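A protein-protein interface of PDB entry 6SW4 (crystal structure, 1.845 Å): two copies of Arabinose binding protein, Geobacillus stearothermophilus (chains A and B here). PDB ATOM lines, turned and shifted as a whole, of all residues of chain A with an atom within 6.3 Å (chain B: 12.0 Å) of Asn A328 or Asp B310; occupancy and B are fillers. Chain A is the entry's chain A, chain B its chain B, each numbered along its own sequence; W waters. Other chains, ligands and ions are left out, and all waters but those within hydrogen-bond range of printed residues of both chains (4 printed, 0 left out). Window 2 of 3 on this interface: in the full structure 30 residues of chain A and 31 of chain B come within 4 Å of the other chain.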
ATOM      1  N   ARG A  63     -19.888 -13.876 -29.936  1.00  0.00           N
ATOM      2  CA  ARG A  63     -21.087 -13.119 -30.274  1.00  0.00           C
ATOM      3  C   ARG A  63     -20.940 -12.378 -31.603  1.00  0.00           C
ATOM      4  O   ARG A  63     -21.939 -12.124 -32.277  1.00  0.00           O
ATOM      5  CB  ARG A  63     -21.433 -12.142 -29.153  1.00  0.00           C
ATOM      6  CG  ARG A  63     -22.785 -11.470 -29.294  1.00  0.00           C
ATOM      7  CD  ARG A  63     -23.427 -11.209 -27.933  1.00  0.00           C
ATOM      8  NE  ARG A  63     -22.534 -10.505 -27.023  1.00  0.00           N
ATOM      9  CZ  ARG A  63     -22.040 -11.007 -25.887  1.00  0.00           C
ATOM     10  NH1 ARG A  63     -22.350 -12.234 -25.485  1.00  0.00           N
ATOM     11  NH2 ARG A  63     -21.233 -10.262 -25.136  1.00  0.00           N
ATOM     12  N   THR A 322     -23.289  -1.320 -24.623  1.00  0.00           N
ATOM     13  CA  THR A 322     -24.306  -1.609 -23.635  1.00  0.00           C
ATOM     14  C   THR A 322     -23.671  -1.606 -22.260  1.00  0.00           C
ATOM     15  O   THR A 322     -22.641  -2.254 -22.049  1.00  0.00           O
ATOM     16  CB  THR A 322     -24.977  -2.957 -23.907  1.00  0.00           C
ATOM     17  OG1 THR A 322     -25.442  -2.981 -25.265  1.00  0.00           O
ATOM     18  CG2 THR A 322     -26.155  -3.133 -22.970  1.00  0.00           C
ATOM     19  N   VAL A 323     -24.300  -0.897 -21.334  1.00  0.00           N
ATOM     20  CA  VAL A 323     -23.900  -0.965 -19.939  1.00  0.00           C
ATOM     21  C   VAL A 323     -24.459  -2.250 -19.361  1.00  0.00           C
ATOM     22  O   VAL A 323     -25.676  -2.431 -19.310  1.00  0.00           O
ATOM     23  CB  VAL A 323     -24.393   0.247 -19.142  1.00  0.00           C
ATOM     24  CG1 VAL A 323     -23.816   0.196 -17.725  1.00  0.00           C
ATOM     25  CG2 VAL A 323     -23.983   1.561 -19.830  1.00  0.00           C
ATOM     26  N   VAL A 324     -23.566  -3.106 -18.868  1.00  0.00           N
ATOM     27  CA  VAL A 324     -23.915  -4.385 -18.279  1.00  0.00           C
ATOM     28  C   VAL A 324     -23.831  -4.226 -16.774  1.00  0.00           C
ATOM     29  O   VAL A 324     -22.776  -3.868 -16.241  1.00  0.00           O
ATOM     30  CB  VAL A 324     -22.975  -5.483 -18.774  1.00  0.00           C
ATOM     31  CG1 VAL A 324     -23.329  -6.816 -18.177  1.00  0.00           C
ATOM     32  CG2 VAL A 324     -23.041  -5.560 -20.295  1.00  0.00           C
ATOM     33  N   THR A 325     -24.944  -4.510 -16.085  1.00  0.00           N
ATOM     34  CA  THR A 325     -24.999  -4.450 -14.632  1.00  0.00           C
ATOM     35  C   THR A 325     -25.587  -5.766 -14.125  1.00  0.00           C
ATOM     36  O   THR A 325     -25.860  -6.665 -14.920  1.00  0.00           O
ATOM     37  CB  THR A 325     -25.856  -3.271 -14.151  1.00  0.00           C
ATOM     38  OG1 THR A 325     -27.223  -3.537 -14.477  1.00  0.00           O
ATOM     39  CG2 THR A 325     -25.418  -1.931 -14.815  1.00  0.00           C
ATOM     40  N   ARG A 326     -25.827  -5.876 -12.815  1.00  0.00           N
ATOM     41  CA  ARG A 326     -26.473  -7.084 -12.289  1.00  0.00           C
ATOM     42  C   ARG A 326     -27.802  -7.382 -12.971  1.00  0.00           C
ATOM     43  O   ARG A 326     -28.234  -8.544 -13.005  1.00  0.00           O
ATOM     44  CB  ARG A 326     -26.693  -6.945 -10.789  1.00  0.00           C
ATOM     45  CG  ARG A 326     -25.601  -7.556  -9.999  1.00  0.00           C
ATOM     46  CD  ARG A 326     -25.760  -7.153  -8.566  1.00  0.00           C
ATOM     47  NE  ARG A 326     -25.392  -8.248  -7.694  1.00  0.00           N
ATOM     48  CZ  ARG A 326     -24.914  -8.077  -6.472  1.00  0.00           C
ATOM     49  NH1 ARG A 326     -24.751  -6.843  -6.010  1.00  0.00           N
ATOM     50  NH2 ARG A 326     -24.601  -9.136  -5.727  1.00  0.00           N
ATOM     51  N   ASP A 327     -28.461  -6.361 -13.513  1.00  0.00           N
ATOM     52  CA  ASP A 327     -29.789  -6.521 -14.087  1.00  0.00           C
ATOM     53  C   ASP A 327     -29.776  -7.277 -15.409  1.00  0.00           C
ATOM     54  O   ASP A 327     -30.763  -7.936 -15.745  1.00  0.00           O
ATOM     55  CB  ASP A 327     -30.439  -5.158 -14.318  1.00  0.00           C
ATOM     56  CG  ASP A 327     -30.710  -4.409 -13.036  1.00  0.00           C
ATOM     57  OD1 ASP A 327     -30.617  -5.009 -11.947  1.00  0.00           O
ATOM     58  OD2 ASP A 327     -31.023  -3.209 -13.132  1.00  0.00           O
ATOM     59  N   ASN A 328     -28.726  -7.126 -16.221  1.00  0.00           N
ATOM     60  CA  ASN A 328     -28.678  -7.793 -17.510  1.00  0.00           C
ATOM     61  C   ASN A 328     -27.429  -8.647 -17.687  1.00  0.00           C
ATOM     62  O   ASN A 328     -27.216  -9.177 -18.779  1.00  0.00           O
ATOM     63  CB  ASN A 328     -28.774  -6.777 -18.662  1.00  0.00           C
ATOM     64  CG  ASN A 328     -27.720  -5.700 -18.565  1.00  0.00           C
ATOM     65  OD1 ASN A 328     -27.062  -5.592 -17.553  1.00  0.00           O
ATOM     66  ND2 ASN A 328     -27.560  -4.909 -19.614  1.00  0.00           N
ATOM     67  N   VAL A 329     -26.613  -8.812 -16.646  1.00  0.00           N
ATOM     68  CA  VAL A 329     -25.371  -9.564 -16.791  1.00  0.00           C
ATOM     69  C   VAL A 329     -25.640 -10.949 -17.377  1.00  0.00           C
ATOM     70  O   VAL A 329     -24.881 -11.440 -18.225  1.00  0.00           O
ATOM     71  CB  VAL A 329     -24.631  -9.636 -15.437  1.00  0.00           C
ATOM     72  CG1 VAL A 329     -25.390 -10.477 -14.413  1.00  0.00           C
ATOM     73  CG2 VAL A 329     -23.219 -10.164 -15.629  1.00  0.00           C
ATOM     74  N   ASP A 330     -26.757 -11.578 -16.988  1.00  0.00           N
ATOM     75  CA  ASP A 330     -27.009 -12.940 -17.451  1.00  0.00           C
ATOM     76  C   ASP A 330     -27.093 -13.013 -18.967  1.00  0.00           C
ATOM     77  O   ASP A 330     -26.749 -14.039 -19.554  1.00  0.00           O
ATOM     78  CB  ASP A 330     -28.284 -13.493 -16.817  1.00  0.00           C
ATOM     79  CG  ASP A 330     -28.070 -13.899 -15.381  1.00  0.00           C
ATOM     80  OD1 ASP A 330     -26.928 -14.285 -15.049  1.00  0.00           O
ATOM     81  OD2 ASP A 330     -29.031 -13.844 -14.585  1.00  0.00           O
ATOM     82  N   HIS A 331     -27.504 -11.929 -19.620  1.00  0.00           N
ATOM     83  CA  HIS A 331     -27.633 -11.940 -21.074  1.00  0.00           C
ATOM     84  C   HIS A 331     -26.297 -11.980 -21.803  1.00  0.00           C
ATOM     85  O   HIS A 331     -26.307 -12.134 -23.027  1.00  0.00           O
ATOM     86  CB  HIS A 331     -28.414 -10.711 -21.560  1.00  0.00           C
ATOM     87  CG  HIS A 331     -29.712 -10.472 -20.840  1.00  0.00           C
ATOM     88  ND1 HIS A 331     -30.852 -10.046 -21.490  1.00  0.00           N
ATOM     89  CD2 HIS A 331     -30.042 -10.564 -19.527  1.00  0.00           C
ATOM     90  CE1 HIS A 331     -31.831  -9.906 -20.612  1.00  0.00           C
ATOM     91  NE2 HIS A 331     -31.364 -10.209 -19.414  1.00  0.00           N
ATOM     92  N   PHE A 332     -25.158 -11.836 -21.112  1.00  0.00           N
ATOM     93  CA  PHE A 332     -23.879 -11.623 -21.787  1.00  0.00           C
ATOM     94  C   PHE A 332     -22.869 -12.752 -21.636  1.00  0.00           C
ATOM     95  O   PHE A 332     -21.783 -12.653 -22.220  1.00  0.00           O
ATOM     96  CB  PHE A 332     -23.253 -10.302 -21.310  1.00  0.00           C
ATOM     97  CG  PHE A 332     -24.037  -9.129 -21.734  1.00  0.00           C
ATOM     98  CD1 PHE A 332     -23.790  -8.530 -22.958  1.00  0.00           C
ATOM     99  CD2 PHE A 332     -25.083  -8.663 -20.951  1.00  0.00           C
ATOM    100  CE1 PHE A 332     -24.555  -7.461 -23.377  1.00  0.00           C
ATOM    101  CE2 PHE A 332     -25.846  -7.595 -21.367  1.00  0.00           C
ATOM    102  CZ  PHE A 332     -25.586  -6.995 -22.580  1.00  0.00           C
ATOM    103  N   PHE B 144     -33.688   6.058 -33.441  1.00  0.00           N
ATOM    104  CA  PHE B 144     -32.808   4.933 -33.160  1.00  0.00           C
ATOM    105  C   PHE B 144     -31.431   5.063 -33.817  1.00  0.00           C
ATOM    106  O   PHE B 144     -30.459   4.474 -33.316  1.00  0.00           O
ATOM    107  CB  PHE B 144     -33.499   3.640 -33.600  1.00  0.00           C
ATOM    108  CG  PHE B 144     -34.882   3.448 -33.008  1.00  0.00           C
ATOM    109  CD1 PHE B 144     -36.006   4.002 -33.614  1.00  0.00           C
ATOM    110  CD2 PHE B 144     -35.058   2.707 -31.852  1.00  0.00           C
ATOM    111  CE1 PHE B 144     -37.277   3.819 -33.079  1.00  0.00           C
ATOM    112  CE2 PHE B 144     -36.331   2.515 -31.314  1.00  0.00           C
ATOM    113  CZ  PHE B 144     -37.440   3.074 -31.936  1.00  0.00           C
ATOM    114  N   LEU B 298     -35.917  -2.585 -38.051  1.00  0.00           N
ATOM    115  CA  LEU B 298     -36.642  -2.141 -36.870  1.00  0.00           C
ATOM    116  C   LEU B 298     -38.098  -2.582 -36.918  1.00  0.00           C
ATOM    117  O   LEU B 298     -38.644  -3.052 -35.913  1.00  0.00           O
ATOM    118  CB  LEU B 298     -36.545  -0.626 -36.768  1.00  0.00           C
ATOM    119  CG  LEU B 298     -36.175   0.052 -35.445  1.00  0.00           C
ATOM    120  CD1 LEU B 298     -35.053  -0.668 -34.762  1.00  0.00           C
ATOM    121  CD2 LEU B 298     -35.756   1.471 -35.731  1.00  0.00           C
ATOM    122  N   HIS B 301     -38.406  -6.210 -36.303  1.00  0.00           N
ATOM    123  CA  HIS B 301     -37.766  -6.598 -35.044  1.00  0.00           C
ATOM    124  C   HIS B 301     -36.716  -7.683 -35.268  1.00  0.00           C
ATOM    125  O   HIS B 301     -36.721  -8.743 -34.627  1.00  0.00           O
ATOM    126  CB  HIS B 301     -38.813  -7.034 -34.012  1.00  0.00           C
ATOM    127  CG  HIS B 301     -39.755  -5.935 -33.620  1.00  0.00           C
ATOM    128  ND1 HIS B 301     -40.973  -5.740 -34.240  1.00  0.00           N
ATOM    129  CD2 HIS B 301     -39.645  -4.953 -32.691  1.00  0.00           C
ATOM    130  CE1 HIS B 301     -41.576  -4.694 -33.704  1.00  0.00           C
ATOM    131  NE2 HIS B 301     -40.792  -4.198 -32.761  1.00  0.00           N
ATOM    132  N   LEU B 302     -35.804  -7.400 -36.201  1.00  0.00           N
ATOM    133  CA  LEU B 302     -34.753  -8.327 -36.594  1.00  0.00           C
ATOM    134  C   LEU B 302     -33.479  -8.158 -35.783  1.00  0.00           C
ATOM    135  O   LEU B 302     -32.519  -8.910 -35.991  1.00  0.00           O
ATOM    136  CB  LEU B 302     -34.441  -8.159 -38.079  1.00  0.00           C
ATOM    137  CG  LEU B 302     -35.579  -8.533 -39.024  1.00  0.00           C
ATOM    138  CD1 LEU B 302     -35.180  -8.193 -40.446  1.00  0.00           C
ATOM    139  CD2 LEU B 302     -35.899 -10.026 -38.896  1.00  0.00           C
ATOM    140  N   THR B 303     -33.428  -7.191 -34.876  1.00  0.00           N
ATOM    141  CA  THR B 303     -32.307  -7.122 -33.945  1.00  0.00           C
ATOM    142  C   THR B 303     -32.736  -7.871 -32.679  1.00  0.00           C
ATOM    143  O   THR B 303     -33.273  -7.308 -31.718  1.00  0.00           O
ATOM    144  CB  THR B 303     -31.869  -5.675 -33.711  1.00  0.00           C
ATOM    145  OG1 THR B 303     -31.000  -5.614 -32.572  1.00  0.00           O
ATOM    146  CG2 THR B 303     -33.059  -4.696 -33.550  1.00  0.00           C
ATOM    147  N   SER B 304     -32.491  -9.190 -32.731  1.00  0.00           N
ATOM    148  CA  SER B 304     -32.849 -10.182 -31.724  1.00  0.00           C
ATOM    149  C   SER B 304     -32.675  -9.644 -30.282  1.00  0.00           C
ATOM    150  O   SER B 304     -31.758  -8.858 -30.043  1.00  0.00           O
ATOM    151  CB  SER B 304     -31.966 -11.421 -31.912  1.00  0.00           C
ATOM    152  OG  SER B 304     -31.743 -12.105 -30.687  1.00  0.00           O
ATOM    153  N   PRO B 305     -33.535 -10.006 -29.360  1.00  0.00           N
ATOM    154  CA  PRO B 305     -33.230  -9.781 -27.933  1.00  0.00           C
ATOM    155  C   PRO B 305     -32.650 -10.994 -27.224  1.00  0.00           C
ATOM    156  O   PRO B 305     -32.319 -10.882 -26.038  1.00  0.00           O
ATOM    157  CB  PRO B 305     -34.616  -9.436 -27.367  1.00  0.00           C
ATOM    158  CG  PRO B 305     -35.566 -10.317 -28.149  1.00  0.00           C
ATOM    159  CD  PRO B 305     -34.911 -10.513 -29.531  1.00  0.00           C
ATOM    160  N   SER B 306     -32.498 -12.127 -27.917  1.00  0.00           N
ATOM    161  CA  SER B 306     -31.990 -13.360 -27.327  1.00  0.00           C
ATOM    162  C   SER B 306     -30.647 -13.728 -27.948  1.00  0.00           C
ATOM    163  O   SER B 306     -30.550 -13.897 -29.172  1.00  0.00           O
ATOM    164  CB  SER B 306     -32.998 -14.507 -27.502  1.00  0.00           C
ATOM    165  OG  SER B 306     -33.704 -14.415 -28.732  1.00  0.00           O
ATOM    166  N   ARG B 307     -29.625 -13.881 -27.090  1.00  0.00           N
ATOM    167  CA  ARG B 307     -28.235 -14.182 -27.464  1.00  0.00           C
ATOM    168  C   ARG B 307     -27.595 -13.049 -28.286  1.00  0.00           C
ATOM    169  O   ARG B 307     -26.569 -13.245 -28.951  1.00  0.00           O
ATOM    170  CB  ARG B 307     -28.123 -15.527 -28.202  1.00  0.00           C
ATOM    171  CG  ARG B 307     -28.504 -16.764 -27.371  1.00  0.00           C
ATOM    172  CD  ARG B 307     -27.482 -17.905 -27.533  1.00  0.00           C
ATOM    173  NE  ARG B 307     -27.473 -18.829 -26.394  1.00  0.00           N
ATOM    174  CZ  ARG B 307     -26.915 -18.562 -25.214  1.00  0.00           C
ATOM    175  NH1 ARG B 307     -26.330 -17.387 -25.007  1.00  0.00           N
ATOM    176  NH2 ARG B 307     -26.949 -19.463 -24.234  1.00  0.00           N
ATOM    177  N   SER B 308     -28.164 -11.848 -28.200  1.00  0.00           N
ATOM    178  CA  SER B 308     -27.751 -10.671 -28.955  1.00  0.00           C
ATOM    179  C   SER B 308     -26.918  -9.694 -28.127  1.00  0.00           C
ATOM    180  O   SER B 308     -26.512  -8.645 -28.643  1.00  0.00           O
ATOM    181  CB  SER B 308     -28.997  -9.976 -29.510  1.00  0.00           C
ATOM    182  OG  SER B 308     -28.820  -8.589 -29.680  1.00  0.00           O
ATOM    183  N   GLY B 309     -26.644 -10.016 -26.864  1.00  0.00           N
ATOM    184  CA  GLY B 309     -26.047  -9.032 -25.977  1.00  0.00           C
ATOM    185  C   GLY B 309     -26.913  -7.791 -25.865  1.00  0.00           C
ATOM    186  O   GLY B 309     -26.402  -6.680 -25.675  1.00  0.00           O
ATOM    187  N   ASP B 310     -28.231  -7.985 -26.008  1.00  0.00           N
ATOM    188  CA  ASP B 310     -29.231  -6.926 -25.855  1.00  0.00           C
ATOM    189  C   ASP B 310     -28.881  -5.696 -26.684  1.00  0.00           C
ATOM    190  O   ASP B 310     -29.029  -4.558 -26.234  1.00  0.00           O
ATOM    191  CB  ASP B 310     -29.402  -6.540 -24.388  1.00  0.00           C
ATOM    192  CG  ASP B 310     -29.936  -7.675 -23.536  1.00  0.00           C
ATOM    193  OD1 ASP B 310     -30.636  -8.566 -24.066  1.00  0.00           O
ATOM    194  OD2 ASP B 310     -29.659  -7.662 -22.322  1.00  0.00           O
ATOM    195  N   ALA B 311     -28.405  -5.918 -27.901  1.00  0.00           N
ATOM    196  CA  ALA B 311     -28.059  -4.789 -28.741  1.00  0.00           C
ATOM    197  C   ALA B 311     -29.307  -4.073 -29.258  1.00  0.00           C
ATOM    198  O   ALA B 311     -30.415  -4.636 -29.304  1.00  0.00           O
ATOM    199  CB  ALA B 311     -27.190  -5.248 -29.904  1.00  0.00           C
ATOM    200  N   LEU B 312     -29.107  -2.800 -29.621  1.00  0.00           N
ATOM    201  CA  LEU B 312     -30.019  -1.954 -30.386  1.00  0.00           C
ATOM    202  C   LEU B 312     -29.445  -1.758 -31.779  1.00  0.00           C
ATOM    203  O   LEU B 312     -28.325  -2.174 -32.052  1.00  0.00           O
ATOM    204  CB  LEU B 312     -30.199  -0.587 -29.732  1.00  0.00           C
ATOM    205  CG  LEU B 312     -31.106  -0.356 -28.530  1.00  0.00           C
ATOM    206  CD1 LEU B 312     -31.104  -1.534 -27.556  1.00  0.00           C
ATOM    207  CD2 LEU B 312     -30.628   0.879 -27.852  1.00  0.00           C
ATOM    208  N   LEU B 313     -30.225  -1.103 -32.649  1.00  0.00           N
ATOM    209  CA  LEU B 313     -29.727  -0.638 -33.943  1.00  0.00           C
ATOM    210  C   LEU B 313     -28.419   0.141 -33.796  1.00  0.00           C
ATOM    211  O   LEU B 313     -28.257   0.899 -32.830  1.00  0.00           O
ATOM    212  CB  LEU B 313     -30.742   0.295 -34.616  1.00  0.00           C
ATOM    213  CG  LEU B 313     -31.563  -0.041 -35.850  1.00  0.00           C
ATOM    214  CD1 LEU B 313     -32.083   1.250 -36.428  1.00  0.00           C
ATOM    215  CD2 LEU B 313     -30.818  -0.904 -36.882  1.00  0.00           C
ATOM    216  N   PRO B 314     -27.493   0.046 -34.756  1.00  0.00           N
ATOM    217  CA  PRO B 314     -26.355   0.974 -34.761  1.00  0.00           C
ATOM    218  C   PRO B 314     -26.834   2.411 -34.696  1.00  0.00           C
ATOM    219  O   PRO B 314     -27.718   2.821 -35.446  1.00  0.00           O
ATOM    220  CB  PRO B 314     -25.656   0.673 -36.086  1.00  0.00           C
ATOM    221  CG  PRO B 314     -25.904  -0.767 -36.295  1.00  0.00           C
ATOM    222  CD  PRO B 314     -27.300  -1.042 -35.732  1.00  0.00           C
ATOM    223  N   ALA B 315     -26.273   3.165 -33.761  1.00  0.00           N
ATOM    224  CA  ALA B 315     -26.746   4.525 -33.529  1.00  0.00           C
ATOM    225  C   ALA B 315     -26.130   5.538 -34.485  1.00  0.00           C
ATOM    226  O   ALA B 315     -26.632   6.657 -34.576  1.00  0.00           O
ATOM    227  CB  ALA B 315     -26.459   4.946 -32.091  1.00  0.00           C
HETATM  228  O   HOH W   1     -23.800  -7.779 -28.763  1.00  0.00           O
HETATM  229  O   HOH W   2     -29.457  -5.079 -21.667  1.00  0.00           O
HETATM  230  O   HOH W   3     -26.810 -12.292 -25.377  1.00  0.00           O
HETATM  231  O   HOH W   4     -28.279  -2.371 -25.576  1.00  0.00           O
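Among the printed residues, merely in contact across the chains: Phe A332 with Gly B309 (3.0 Å), Arg A63 with Gly B309 (3.6 Å), Arg A63 with Ser B308 (3.8 Å), Thr A322 with Gly B309 (3.8 Å), Asn A328 with Asp B310 (3.9 Å), Arg A63 with Arg B307 (3.9 Å) and Phe A332 with Asp B310 (3.9 Å).
Water W4 lies within hydrogen-bond range of O of Asp B310 (2.4 Å) and OG1 of Thr A322 (2.9 Å). Water W3 lies within hydrogen-bond range of the backbone carbonyl oxygen of His A331 (2.4 Å), the backbone NH of Gly B309 (2.7 Å) and the backbone NH of Ser B308 (3.2 Å). Water W2 bridges OD2 of Asp B310 (2.7 Å) and ND2 of Asn A328 (2.8 Å). Water W1 lies within hydrogen-bond range of the backbone carbonyl oxygen of Ser B308 and the guanidinium group of Arg A63.
Of the 12 printed residues of chain A, 5 touch a printed residue of chain B. Of the 17 printed residues of chain B, 4 touch a printed residue of chain A. Among the printed residues, 8 pairs touch across the chains.
The guanidinium group (NH1) of Arg A63 sits at hydrogen-bond distance from the backbone carbonyl oxygen (O) of Phe A332 (3.3 Å). The backbone carbonyl oxygen (O) of Val A323 sits at hydrogen-bond distance from the side-chain amide nitrogen (ND2) of Asn A328 (3.1 Å). OD1 of Asn A328 sits at hydrogen-bond distance from N of Thr A325. The side-chain hydroxyl (OG) of Ser B308 lies within hydrogen-bond range of the backbone carbonyl oxygen (O) of Ser B304 (3.0 Å). The side-chain hydroxyl (OG) of Ser B308 lies within hydrogen-bond range of the backbone NH (N) of Ala B311 (3.2 Å).
No position is printed for both chains. Of the 8 pairs that touch across the chains among the printed residues, none has its exchanged pair printed and touching as well.
ND1 of His A331 lies within hydrogen-bond range of OD2 of Asp B310, at 2.8 Å.
Of chain B, only Asp B310 comes within 4 Å of Asn A328. Of chain A, only Asn A328 (3.9 Å), His A331 (2.8 Å) and Phe A332 (3.9 Å) come within 4 Å of Asp B310. Thr A322 touches one residue of chain B. No residue of chain B comes within 4 Å of Val A323. No residue of chain B comes within 4 Å of Val A324. No residue of chain B comes within 4 Å of Thr A325. No residue of chain B comes within 4 Å of Val A329. Phe A332 touches just these residues of chain B: Gly B309 and Asp B310. Of the printed residues of chain B, Arg A63 touches Arg B307 (3.9 Å), Ser B308 (3.8 Å) and Gly B309 (3.6 Å). Printed residues of chain A within 4 Å of Arg B307: Arg A63 (3.9 Å). Printed residues of chain A within 4 Å of Ser B308: Arg A63 (3.8 Å). Printed residues of chain A within 4 Å of Gly B309: Arg A63 (3.6 Å), Thr A322 (3.8 Å) and Phe A332 (3.0 Å). Leu B298 touches none of the printed residues of chain A. Ser B304 touches none of the printed residues of chain A. The nearest residue of chain A that does not touch Asp B310 is Thr A322 (4.04 Å). The nearest printed residue of chain B that does not touch Arg A63 is Asp B310 (6.1 Å).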
